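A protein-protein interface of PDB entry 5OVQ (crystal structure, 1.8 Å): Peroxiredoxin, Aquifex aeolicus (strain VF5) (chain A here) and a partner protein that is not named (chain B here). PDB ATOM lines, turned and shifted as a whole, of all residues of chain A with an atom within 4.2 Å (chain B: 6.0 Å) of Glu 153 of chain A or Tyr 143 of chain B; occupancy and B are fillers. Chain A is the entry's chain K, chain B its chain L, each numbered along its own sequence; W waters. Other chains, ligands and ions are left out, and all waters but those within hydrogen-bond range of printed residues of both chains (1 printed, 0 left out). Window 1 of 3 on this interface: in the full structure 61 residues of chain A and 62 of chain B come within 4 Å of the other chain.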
ATOM      1  N   ILE A 141      30.817  17.738 -13.556  1.00  0.00           N
ATOM      2  CA  ILE A 141      31.044  19.108 -13.112  1.00  0.00           C
ATOM      3  C   ILE A 141      31.782  19.072 -11.786  1.00  0.00           C
ATOM      4  O   ILE A 141      31.651  18.121 -11.005  1.00  0.00           O
ATOM      5  CB  ILE A 141      29.751  19.951 -12.991  1.00  0.00           C
ATOM      6  CG1 ILE A 141      28.937  19.548 -11.772  1.00  0.00           C
ATOM      7  CG2 ILE A 141      28.926  19.901 -14.292  1.00  0.00           C
ATOM      8  CD1 ILE A 141      27.965  20.635 -11.328  1.00  0.00           C
ATOM      9  N   ASN A 150      23.291  23.731  -9.315  1.00  0.00           N
ATOM     10  CA  ASN A 150      22.001  24.086  -9.914  1.00  0.00           C
ATOM     11  C   ASN A 150      21.278  22.784 -10.244  1.00  0.00           C
ATOM     12  O   ASN A 150      21.652  22.087 -11.195  1.00  0.00           O
ATOM     13  CB  ASN A 150      22.220  24.939 -11.172  1.00  0.00           C
ATOM     14  CG  ASN A 150      20.919  25.417 -11.809  1.00  0.00           C
ATOM     15  OD1 ASN A 150      19.872  24.778 -11.700  1.00  0.00           O
ATOM     16  ND2 ASN A 150      20.990  26.550 -12.494  1.00  0.00           N
ATOM     17  N   ILE A 151      20.261  22.440  -9.452  1.00  0.00           N
ATOM     18  CA  ILE A 151      19.636  21.125  -9.587  1.00  0.00           C
ATOM     19  C   ILE A 151      18.868  21.012 -10.908  1.00  0.00           C
ATOM     20  O   ILE A 151      18.876  19.959 -11.559  1.00  0.00           O
ATOM     21  CB  ILE A 151      18.745  20.832  -8.356  1.00  0.00           C
ATOM     22  CG1 ILE A 151      19.575  20.262  -7.196  1.00  0.00           C
ATOM     23  CG2 ILE A 151      17.667  19.822  -8.687  1.00  0.00           C
ATOM     24  CD1 ILE A 151      20.591  21.211  -6.582  1.00  0.00           C
ATOM     25  N   ARG A 152      18.217  22.094 -11.349  1.00  0.00           N
ATOM     26  CA  ARG A 152      17.490  22.009 -12.614  1.00  0.00           C
ATOM     27  C   ARG A 152      18.426  21.814 -13.796  1.00  0.00           C
ATOM     28  O   ARG A 152      18.054  21.151 -14.767  1.00  0.00           O
ATOM     29  CB  ARG A 152      16.608  23.246 -12.818  1.00  0.00           C
ATOM     30  CG  ARG A 152      15.290  23.128 -12.050  1.00  0.00           C
ATOM     31  CD  ARG A 152      14.438  24.379 -12.120  1.00  0.00           C
ATOM     32  NE  ARG A 152      15.025  25.477 -11.360  1.00  0.00           N
ATOM     33  CZ  ARG A 152      14.344  26.513 -10.886  1.00  0.00           C
ATOM     34  NH1 ARG A 152      13.032  26.604 -11.085  1.00  0.00           N
ATOM     35  NH2 ARG A 152      14.978  27.462 -10.210  1.00  0.00           N
ATOM     36  N   GLU A 153      19.645  22.347 -13.723  1.00  0.00           N
ATOM     37  CA  GLU A 153      20.594  22.104 -14.806  1.00  0.00           C
ATOM     38  C   GLU A 153      21.026  20.646 -14.851  1.00  0.00           C
ATOM     39  O   GLU A 153      21.299  20.116 -15.934  1.00  0.00           O
ATOM     40  CB  GLU A 153      21.819  23.012 -14.663  1.00  0.00           C
ATOM     41  CG  GLU A 153      22.955  22.713 -15.657  1.00  0.00           C
ATOM     42  CD  GLU A 153      22.520  22.850 -17.110  1.00  0.00           C
ATOM     43  OE1 GLU A 153      21.463  23.468 -17.375  1.00  0.00           O
ATOM     44  OE2 GLU A 153      23.240  22.335 -17.987  1.00  0.00           O
ATOM     45  N   VAL A 154      21.091  19.981 -13.692  1.00  0.00           N
ATOM     46  CA  VAL A 154      21.376  18.550 -13.679  1.00  0.00           C
ATOM     47  C   VAL A 154      20.271  17.785 -14.403  1.00  0.00           C
ATOM     48  O   VAL A 154      20.543  16.882 -15.207  1.00  0.00           O
ATOM     49  CB  VAL A 154      21.553  18.063 -12.229  1.00  0.00           C
ATOM     50  CG1 VAL A 154      21.873  16.579 -12.208  1.00  0.00           C
ATOM     51  CG2 VAL A 154      22.609  18.899 -11.517  1.00  0.00           C
ATOM     52  N   ILE A 155      19.011  18.152 -14.146  1.00  0.00           N
ATOM     53  CA  ILE A 155      17.883  17.530 -14.834  1.00  0.00           C
ATOM     54  C   ILE A 155      17.933  17.843 -16.327  1.00  0.00           C
ATOM     55  O   ILE A 155      17.709  16.965 -17.169  1.00  0.00           O
ATOM     56  CB  ILE A 155      16.561  17.994 -14.192  1.00  0.00           C
ATOM     57  CG1 ILE A 155      16.489  17.508 -12.738  1.00  0.00           C
ATOM     58  CG2 ILE A 155      15.360  17.518 -14.987  1.00  0.00           C
ATOM     59  CD1 ILE A 155      15.327  18.108 -11.950  1.00  0.00           C
ATOM     60  N   ARG A 156      18.229  19.096 -16.678  1.00  0.00           N
ATOM     61  CA  ARG A 156      18.310  19.465 -18.089  1.00  0.00           C
ATOM     62  C   ARG A 156      19.405  18.682 -18.790  1.00  0.00           C
ATOM     63  O   ARG A 156      19.238  18.247 -19.938  1.00  0.00           O
ATOM     64  CB  ARG A 156      18.570  20.961 -18.237  1.00  0.00           C
ATOM     65  CG  ARG A 156      18.440  21.459 -19.679  1.00  0.00           C
ATOM     66  CD  ARG A 156      19.075  22.827 -19.828  1.00  0.00           C
ATOM     67  NE  ARG A 156      20.523  22.702 -19.787  1.00  0.00           N
ATOM     68  CZ  ARG A 156      21.286  22.422 -20.839  1.00  0.00           C
ATOM     69  NH1 ARG A 156      20.742  22.252 -22.039  1.00  0.00           N
ATOM     70  NH2 ARG A 156      22.597  22.312 -20.681  1.00  0.00           N
ATOM     71  N   LEU A 157      20.541  18.509 -18.113  1.00  0.00           N
ATOM     72  CA  LEU A 157      21.651  17.756 -18.674  1.00  0.00           C
ATOM     73  C   LEU A 157      21.244  16.315 -18.959  1.00  0.00           C
ATOM     74  O   LEU A 157      21.536  15.775 -20.034  1.00  0.00           O
ATOM     75  CB  LEU A 157      22.831  17.820 -17.710  1.00  0.00           C
ATOM     76  CG  LEU A 157      24.066  17.022 -18.079  1.00  0.00           C
ATOM     77  CD1 LEU A 157      24.525  17.474 -19.462  1.00  0.00           C
ATOM     78  CD2 LEU A 157      25.148  17.229 -17.028  1.00  0.00           C
ATOM     79  N   TRP A 182      12.325  28.734 -15.447  1.00  0.00           N
ATOM     80  CA  TRP A 182      12.918  28.400 -14.155  1.00  0.00           C
ATOM     81  C   TRP A 182      12.824  29.632 -13.270  1.00  0.00           C
ATOM     82  O   TRP A 182      13.532  30.618 -13.498  1.00  0.00           O
ATOM     83  CB  TRP A 182      14.374  27.953 -14.278  1.00  0.00           C
ATOM     84  CG  TRP A 182      14.613  26.767 -15.133  1.00  0.00           C
ATOM     85  CD1 TRP A 182      13.695  26.060 -15.862  1.00  0.00           C
ATOM     86  CD2 TRP A 182      15.879  26.147 -15.367  1.00  0.00           C
ATOM     87  NE1 TRP A 182      14.324  25.033 -16.542  1.00  0.00           N
ATOM     88  CE2 TRP A 182      15.663  25.071 -16.256  1.00  0.00           C
ATOM     89  CE3 TRP A 182      17.175  26.412 -14.926  1.00  0.00           C
ATOM     90  CZ2 TRP A 182      16.696  24.247 -16.694  1.00  0.00           C
ATOM     91  CZ3 TRP A 182      18.208  25.590 -15.370  1.00  0.00           C
ATOM     92  CH2 TRP A 182      17.959  24.523 -16.244  1.00  0.00           C
ATOM     93  N   GLN B 119      35.675  10.220 -26.390  1.00  0.00           N
ATOM     94  CA  GLN B 119      34.870  11.213 -27.091  1.00  0.00           C
ATOM     95  C   GLN B 119      35.507  11.567 -28.423  1.00  0.00           C
ATOM     96  O   GLN B 119      34.874  11.462 -29.481  1.00  0.00           O
ATOM     97  CB  GLN B 119      34.713  12.460 -26.227  1.00  0.00           C
ATOM     98  CG  GLN B 119      33.732  12.268 -25.087  1.00  0.00           C
ATOM     99  CD  GLN B 119      32.330  12.600 -25.533  1.00  0.00           C
ATOM    100  OE1 GLN B 119      31.980  13.772 -25.682  1.00  0.00           O
ATOM    101  NE2 GLN B 119      31.534  11.573 -25.808  1.00  0.00           N
ATOM    102  N   VAL B 125      36.511  18.228 -25.714  1.00  0.00           N
ATOM    103  CA  VAL B 125      35.125  18.152 -25.270  1.00  0.00           C
ATOM    104  C   VAL B 125      34.654  19.564 -24.952  1.00  0.00           C
ATOM    105  O   VAL B 125      35.348  20.549 -25.247  1.00  0.00           O
ATOM    106  CB  VAL B 125      34.949  17.224 -24.052  1.00  0.00           C
ATOM    107  CG1 VAL B 125      35.389  15.808 -24.386  1.00  0.00           C
ATOM    108  CG2 VAL B 125      35.699  17.777 -22.836  1.00  0.00           C
ATOM    109  N   ARG B 126      33.467  19.674 -24.359  1.00  0.00           N
ATOM    110  CA  ARG B 126      32.899  20.974 -24.006  1.00  0.00           C
ATOM    111  C   ARG B 126      33.281  21.319 -22.568  1.00  0.00           C
ATOM    112  O   ARG B 126      32.479  21.256 -21.642  1.00  0.00           O
ATOM    113  CB  ARG B 126      31.388  20.965 -24.195  1.00  0.00           C
ATOM    114  CG  ARG B 126      30.980  20.530 -25.569  1.00  0.00           C
ATOM    115  CD  ARG B 126      29.463  20.672 -25.806  1.00  0.00           C
ATOM    116  NE  ARG B 126      29.217  20.162 -27.143  1.00  0.00           N
ATOM    117  CZ  ARG B 126      29.473  20.871 -28.232  1.00  0.00           C
ATOM    118  NH1 ARG B 126      29.893  22.122 -28.096  1.00  0.00           N
ATOM    119  NH2 ARG B 126      29.298  20.348 -29.441  1.00  0.00           N
ATOM    120  N   ALA B 127      34.541  21.694 -22.403  1.00  0.00           N
ATOM    121  CA  ALA B 127      35.055  22.058 -21.094  1.00  0.00           C
ATOM    122  C   ALA B 127      34.870  23.554 -20.876  1.00  0.00           C
ATOM    123  O   ALA B 127      34.861  24.347 -21.823  1.00  0.00           O
ATOM    124  CB  ALA B 127      36.533  21.662 -20.962  1.00  0.00           C
ATOM    125  N   ILE B 141      33.457  22.543 -15.640  1.00  0.00           N
ATOM    126  CA  ILE B 141      32.472  21.578 -16.116  1.00  0.00           C
ATOM    127  C   ILE B 141      33.000  20.940 -17.393  1.00  0.00           C
ATOM    128  O   ILE B 141      33.760  21.551 -18.154  1.00  0.00           O
ATOM    129  CB  ILE B 141      31.063  22.182 -16.343  1.00  0.00           C
ATOM    130  CG1 ILE B 141      30.954  22.865 -17.699  1.00  0.00           C
ATOM    131  CG2 ILE B 141      30.646  23.122 -15.185  1.00  0.00           C
ATOM    132  CD1 ILE B 141      29.525  23.004 -18.165  1.00  0.00           C
ATOM    133  N   TYR B 142      32.629  19.679 -17.603  1.00  0.00           N
ATOM    134  CA  TYR B 142      32.973  18.950 -18.822  1.00  0.00           C
ATOM    135  C   TYR B 142      31.704  18.321 -19.388  1.00  0.00           C
ATOM    136  O   TYR B 142      31.238  17.298 -18.880  1.00  0.00           O
ATOM    137  CB  TYR B 142      34.028  17.879 -18.564  1.00  0.00           C
ATOM    138  CG  TYR B 142      35.378  18.360 -18.101  1.00  0.00           C
ATOM    139  CD1 TYR B 142      36.435  18.476 -18.998  1.00  0.00           C
ATOM    140  CD2 TYR B 142      35.609  18.695 -16.770  1.00  0.00           C
ATOM    141  CE1 TYR B 142      37.686  18.913 -18.577  1.00  0.00           C
ATOM    142  CE2 TYR B 142      36.860  19.129 -16.344  1.00  0.00           C
ATOM    143  CZ  TYR B 142      37.891  19.223 -17.240  1.00  0.00           C
ATOM    144  OH  TYR B 142      39.122  19.660 -16.810  1.00  0.00           O
ATOM    145  N   TYR B 143      31.160  18.925 -20.454  1.00  0.00           N
ATOM    146  CA  TYR B 143      30.022  18.342 -21.149  1.00  0.00           C
ATOM    147  C   TYR B 143      30.493  17.601 -22.398  1.00  0.00           C
ATOM    148  O   TYR B 143      31.556  17.903 -22.944  1.00  0.00           O
ATOM    149  CB  TYR B 143      29.007  19.431 -21.536  1.00  0.00           C
ATOM    150  CG  TYR B 143      28.051  19.843 -20.417  1.00  0.00           C
ATOM    151  CD1 TYR B 143      28.333  19.540 -19.101  1.00  0.00           C
ATOM    152  CD2 TYR B 143      26.875  20.531 -20.695  1.00  0.00           C
ATOM    153  CE1 TYR B 143      27.479  19.908 -18.079  1.00  0.00           C
ATOM    154  CE2 TYR B 143      25.994  20.911 -19.670  1.00  0.00           C
ATOM    155  CZ  TYR B 143      26.316  20.587 -18.361  1.00  0.00           C
ATOM    156  OH  TYR B 143      25.490  20.938 -17.314  1.00  0.00           O
ATOM    157  N   PRO B 144      29.758  16.604 -22.873  1.00  0.00           N
ATOM    158  CA  PRO B 144      30.206  15.825 -24.029  1.00  0.00           C
ATOM    159  C   PRO B 144      29.910  16.547 -25.340  1.00  0.00           C
ATOM    160  O   PRO B 144      29.285  17.608 -25.376  1.00  0.00           O
ATOM    161  CB  PRO B 144      29.386  14.542 -23.915  1.00  0.00           C
ATOM    162  CG  PRO B 144      28.124  14.991 -23.274  1.00  0.00           C
ATOM    163  CD  PRO B 144      28.541  16.033 -22.272  1.00  0.00           C
ATOM    164  N   LEU B 145      30.371  15.933 -26.434  1.00  0.00           N
ATOM    165  CA  LEU B 145      30.221  16.544 -27.755  1.00  0.00           C
ATOM    166  C   LEU B 145      28.755  16.757 -28.124  1.00  0.00           C
ATOM    167  O   LEU B 145      28.435  17.694 -28.857  1.00  0.00           O
ATOM    168  CB  LEU B 145      30.916  15.689 -28.810  1.00  0.00           C
ATOM    169  CG  LEU B 145      32.411  15.478 -28.558  1.00  0.00           C
ATOM    170  CD1 LEU B 145      33.046  14.617 -29.645  1.00  0.00           C
ATOM    171  CD2 LEU B 145      33.119  16.825 -28.472  1.00  0.00           C
ATOM    172  N   THR B 147      26.209  17.756 -26.301  1.00  0.00           N
ATOM    173  CA  THR B 147      25.324  18.449 -25.368  1.00  0.00           C
ATOM    174  C   THR B 147      25.777  19.879 -25.101  1.00  0.00           C
ATOM    175  O   THR B 147      26.727  20.107 -24.342  1.00  0.00           O
ATOM    176  CB  THR B 147      25.241  17.657 -24.069  1.00  0.00           C
ATOM    177  OG1 THR B 147      24.830  16.323 -24.382  1.00  0.00           O
ATOM    178  CG2 THR B 147      24.231  18.292 -23.136  1.00  0.00           C
ATOM    179  N   GLY B 148      25.055  20.840 -25.671  1.00  0.00           N
ATOM    180  CA  GLY B 148      25.385  22.233 -25.446  1.00  0.00           C
ATOM    181  C   GLY B 148      25.223  22.644 -23.993  1.00  0.00           C
ATOM    182  O   GLY B 148      24.433  22.074 -23.234  1.00  0.00           O
ATOM    183  N   ARG B 149      25.972  23.676 -23.620  1.00  0.00           N
ATOM    184  CA  ARG B 149      26.012  24.187 -22.266  1.00  0.00           C
ATOM    185  C   ARG B 149      24.848  25.147 -21.984  1.00  0.00           C
ATOM    186  O   ARG B 149      24.059  25.516 -22.860  1.00  0.00           O
ATOM    187  CB  ARG B 149      27.364  24.852 -22.015  1.00  0.00           C
ATOM    188  CG  ARG B 149      28.484  23.812 -21.828  1.00  0.00           C
ATOM    189  CD  ARG B 149      29.894  24.362 -22.068  1.00  0.00           C
ATOM    190  NE  ARG B 149      30.153  24.481 -23.497  1.00  0.00           N
ATOM    191  CZ  ARG B 149      31.355  24.527 -24.060  1.00  0.00           C
ATOM    192  NH1 ARG B 149      32.456  24.457 -23.326  1.00  0.00           N
ATOM    193  NH2 ARG B 149      31.449  24.647 -25.376  1.00  0.00           N
ATOM    194  N   ASN B 150      24.735  25.512 -20.714  1.00  0.00           N
ATOM    195  CA  ASN B 150      23.702  26.400 -20.191  1.00  0.00           C
ATOM    196  C   ASN B 150      24.386  27.723 -19.855  1.00  0.00           C
ATOM    197  O   ASN B 150      25.065  27.834 -18.830  1.00  0.00           O
ATOM    198  CB  ASN B 150      23.050  25.764 -18.968  1.00  0.00           C
ATOM    199  CG  ASN B 150      21.946  26.608 -18.388  1.00  0.00           C
ATOM    200  OD1 ASN B 150      21.954  27.823 -18.531  1.00  0.00           O
ATOM    201  ND2 ASN B 150      21.013  25.973 -17.681  1.00  0.00           N
ATOM    202  N   GLU B 153      23.665  29.403 -16.512  1.00  0.00           N
ATOM    203  CA  GLU B 153      24.303  28.779 -15.353  1.00  0.00           C
ATOM    204  C   GLU B 153      25.747  29.239 -15.198  1.00  0.00           C
ATOM    205  O   GLU B 153      26.229  29.392 -14.069  1.00  0.00           O
ATOM    206  CB  GLU B 153      24.234  27.256 -15.449  1.00  0.00           C
ATOM    207  CG  GLU B 153      25.017  26.519 -14.334  1.00  0.00           C
ATOM    208  CD  GLU B 153      24.566  26.871 -12.902  1.00  0.00           C
ATOM    209  OE1 GLU B 153      23.469  27.444 -12.709  1.00  0.00           O
ATOM    210  OE2 GLU B 153      25.326  26.557 -11.953  1.00  0.00           O
HETATM  211  O   HOH W   1      22.050  21.045 -24.614  1.00  0.00           O
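Glu 153 of chain A touches just these residues of chain B: Tyr 143 and Asn 150. Of the printed residues of chain A, Ile 141 of chain B touches Ile 141. Of chain A, only Glu 153, Arg 156 and Leu 157 come within 4 Å of Tyr 143 of chain B. Printed residues of chain A within 4 Å of Thr 147 of chain B: Leu 157 (3.8 Å). Of the printed residues of chain A, Asn 150 of chain B touches Glu 153, Arg 156 and Trp 182. The nearest printed residue of chain B that does not touch Arg 156 of chain A is Thr 147 of chain B (5.0 Å).
Of the 14 printed residues of chain B, 7 touch a printed residue of chain A. Printed residues of chain B that touch a printed residue of chain A: Ile 141, Tyr 143, Thr 147, Gly 148, Arg 149, Asn 150 and Glu 153. Along chain B the printed residues that touch a printed residue of chain A span positions 141 to 153. Among the printed residues, 11 pairs touch across the chains. Among the printed residues, no Asp or Glu carboxylate lies within 4 Å of a Lys or Arg side-chain nitrogen of the other chain.
NH2 of Arg 156 of chain A lies within hydrogen-bond range of O of Gly 148 of chain B, at 3.2 Å. The side-chain carboxylate of Glu 153 of chain A sits at hydrogen-bond distance from the side-chain amide nitrogen of Asn 150 of chain B (2.6 Å). OH of Tyr 143 of chain B lies within hydrogen-bond range of OE2 of Glu 153 of chain A (2.7 Å). The side-chain amide nitrogen of Asn 150 of chain A is in hydrogen-bond range of the side-chain carboxylate of Glu 153 of chain B.
Water W1 lies within hydrogen-bond range of the backbone carbonyl oxygen of Gly 148 of chain B and the guanidinium group of Arg 156 of chain A.
The side-chain amide oxygen (OD1) of Asn 150 of chain A lies within hydrogen-bond range of the backbone NH (N) of Arg 152 of chain A, 3.2 Å away. N of Glu 153 of chain B lies within hydrogen-bond range of OD1 of Asn 150 of chain B (3.1 Å). O of Ala 127 of chain B sits at hydrogen-bond distance from NH1 of Arg 149 of chain B (2.8 Å). OD1 of Asn 150 of chain A lies within hydrogen-bond range of N of Glu 153 of chain A, 3.2 Å away. The backbone NH of Tyr 143 of chain B sits at hydrogen-bond distance from the backbone carbonyl oxygen of Arg 126 of chain B. NE of Arg 156 of chain A is in salt-bridge range of OE1 of Glu 153 of chain A, at 2.7 Å.
CG2 of Ile 141 of chain A touches CB of Ile 141 of chain B (3.7 Å). NH2 of Arg 156 of chain A touches CE2 of Tyr 143 of chain B (3.8 Å). Arg 156 of chain A touches Arg 149 of chain B. Asn 150 of chain B touches Arg 156 of chain A (N to NH2, 3.8 Å). CE1 of Tyr 143 of chain B touches CD2 of Leu 157 of chain A, 3.7 Å away. CD1 of Leu 157 of chain A touches CG2 of Thr 147 of chain B, 3.8 Å away. CZ3 of Trp 182 of chain A touches ND2 of Asn 150 of chain B, at 3.7 Å.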
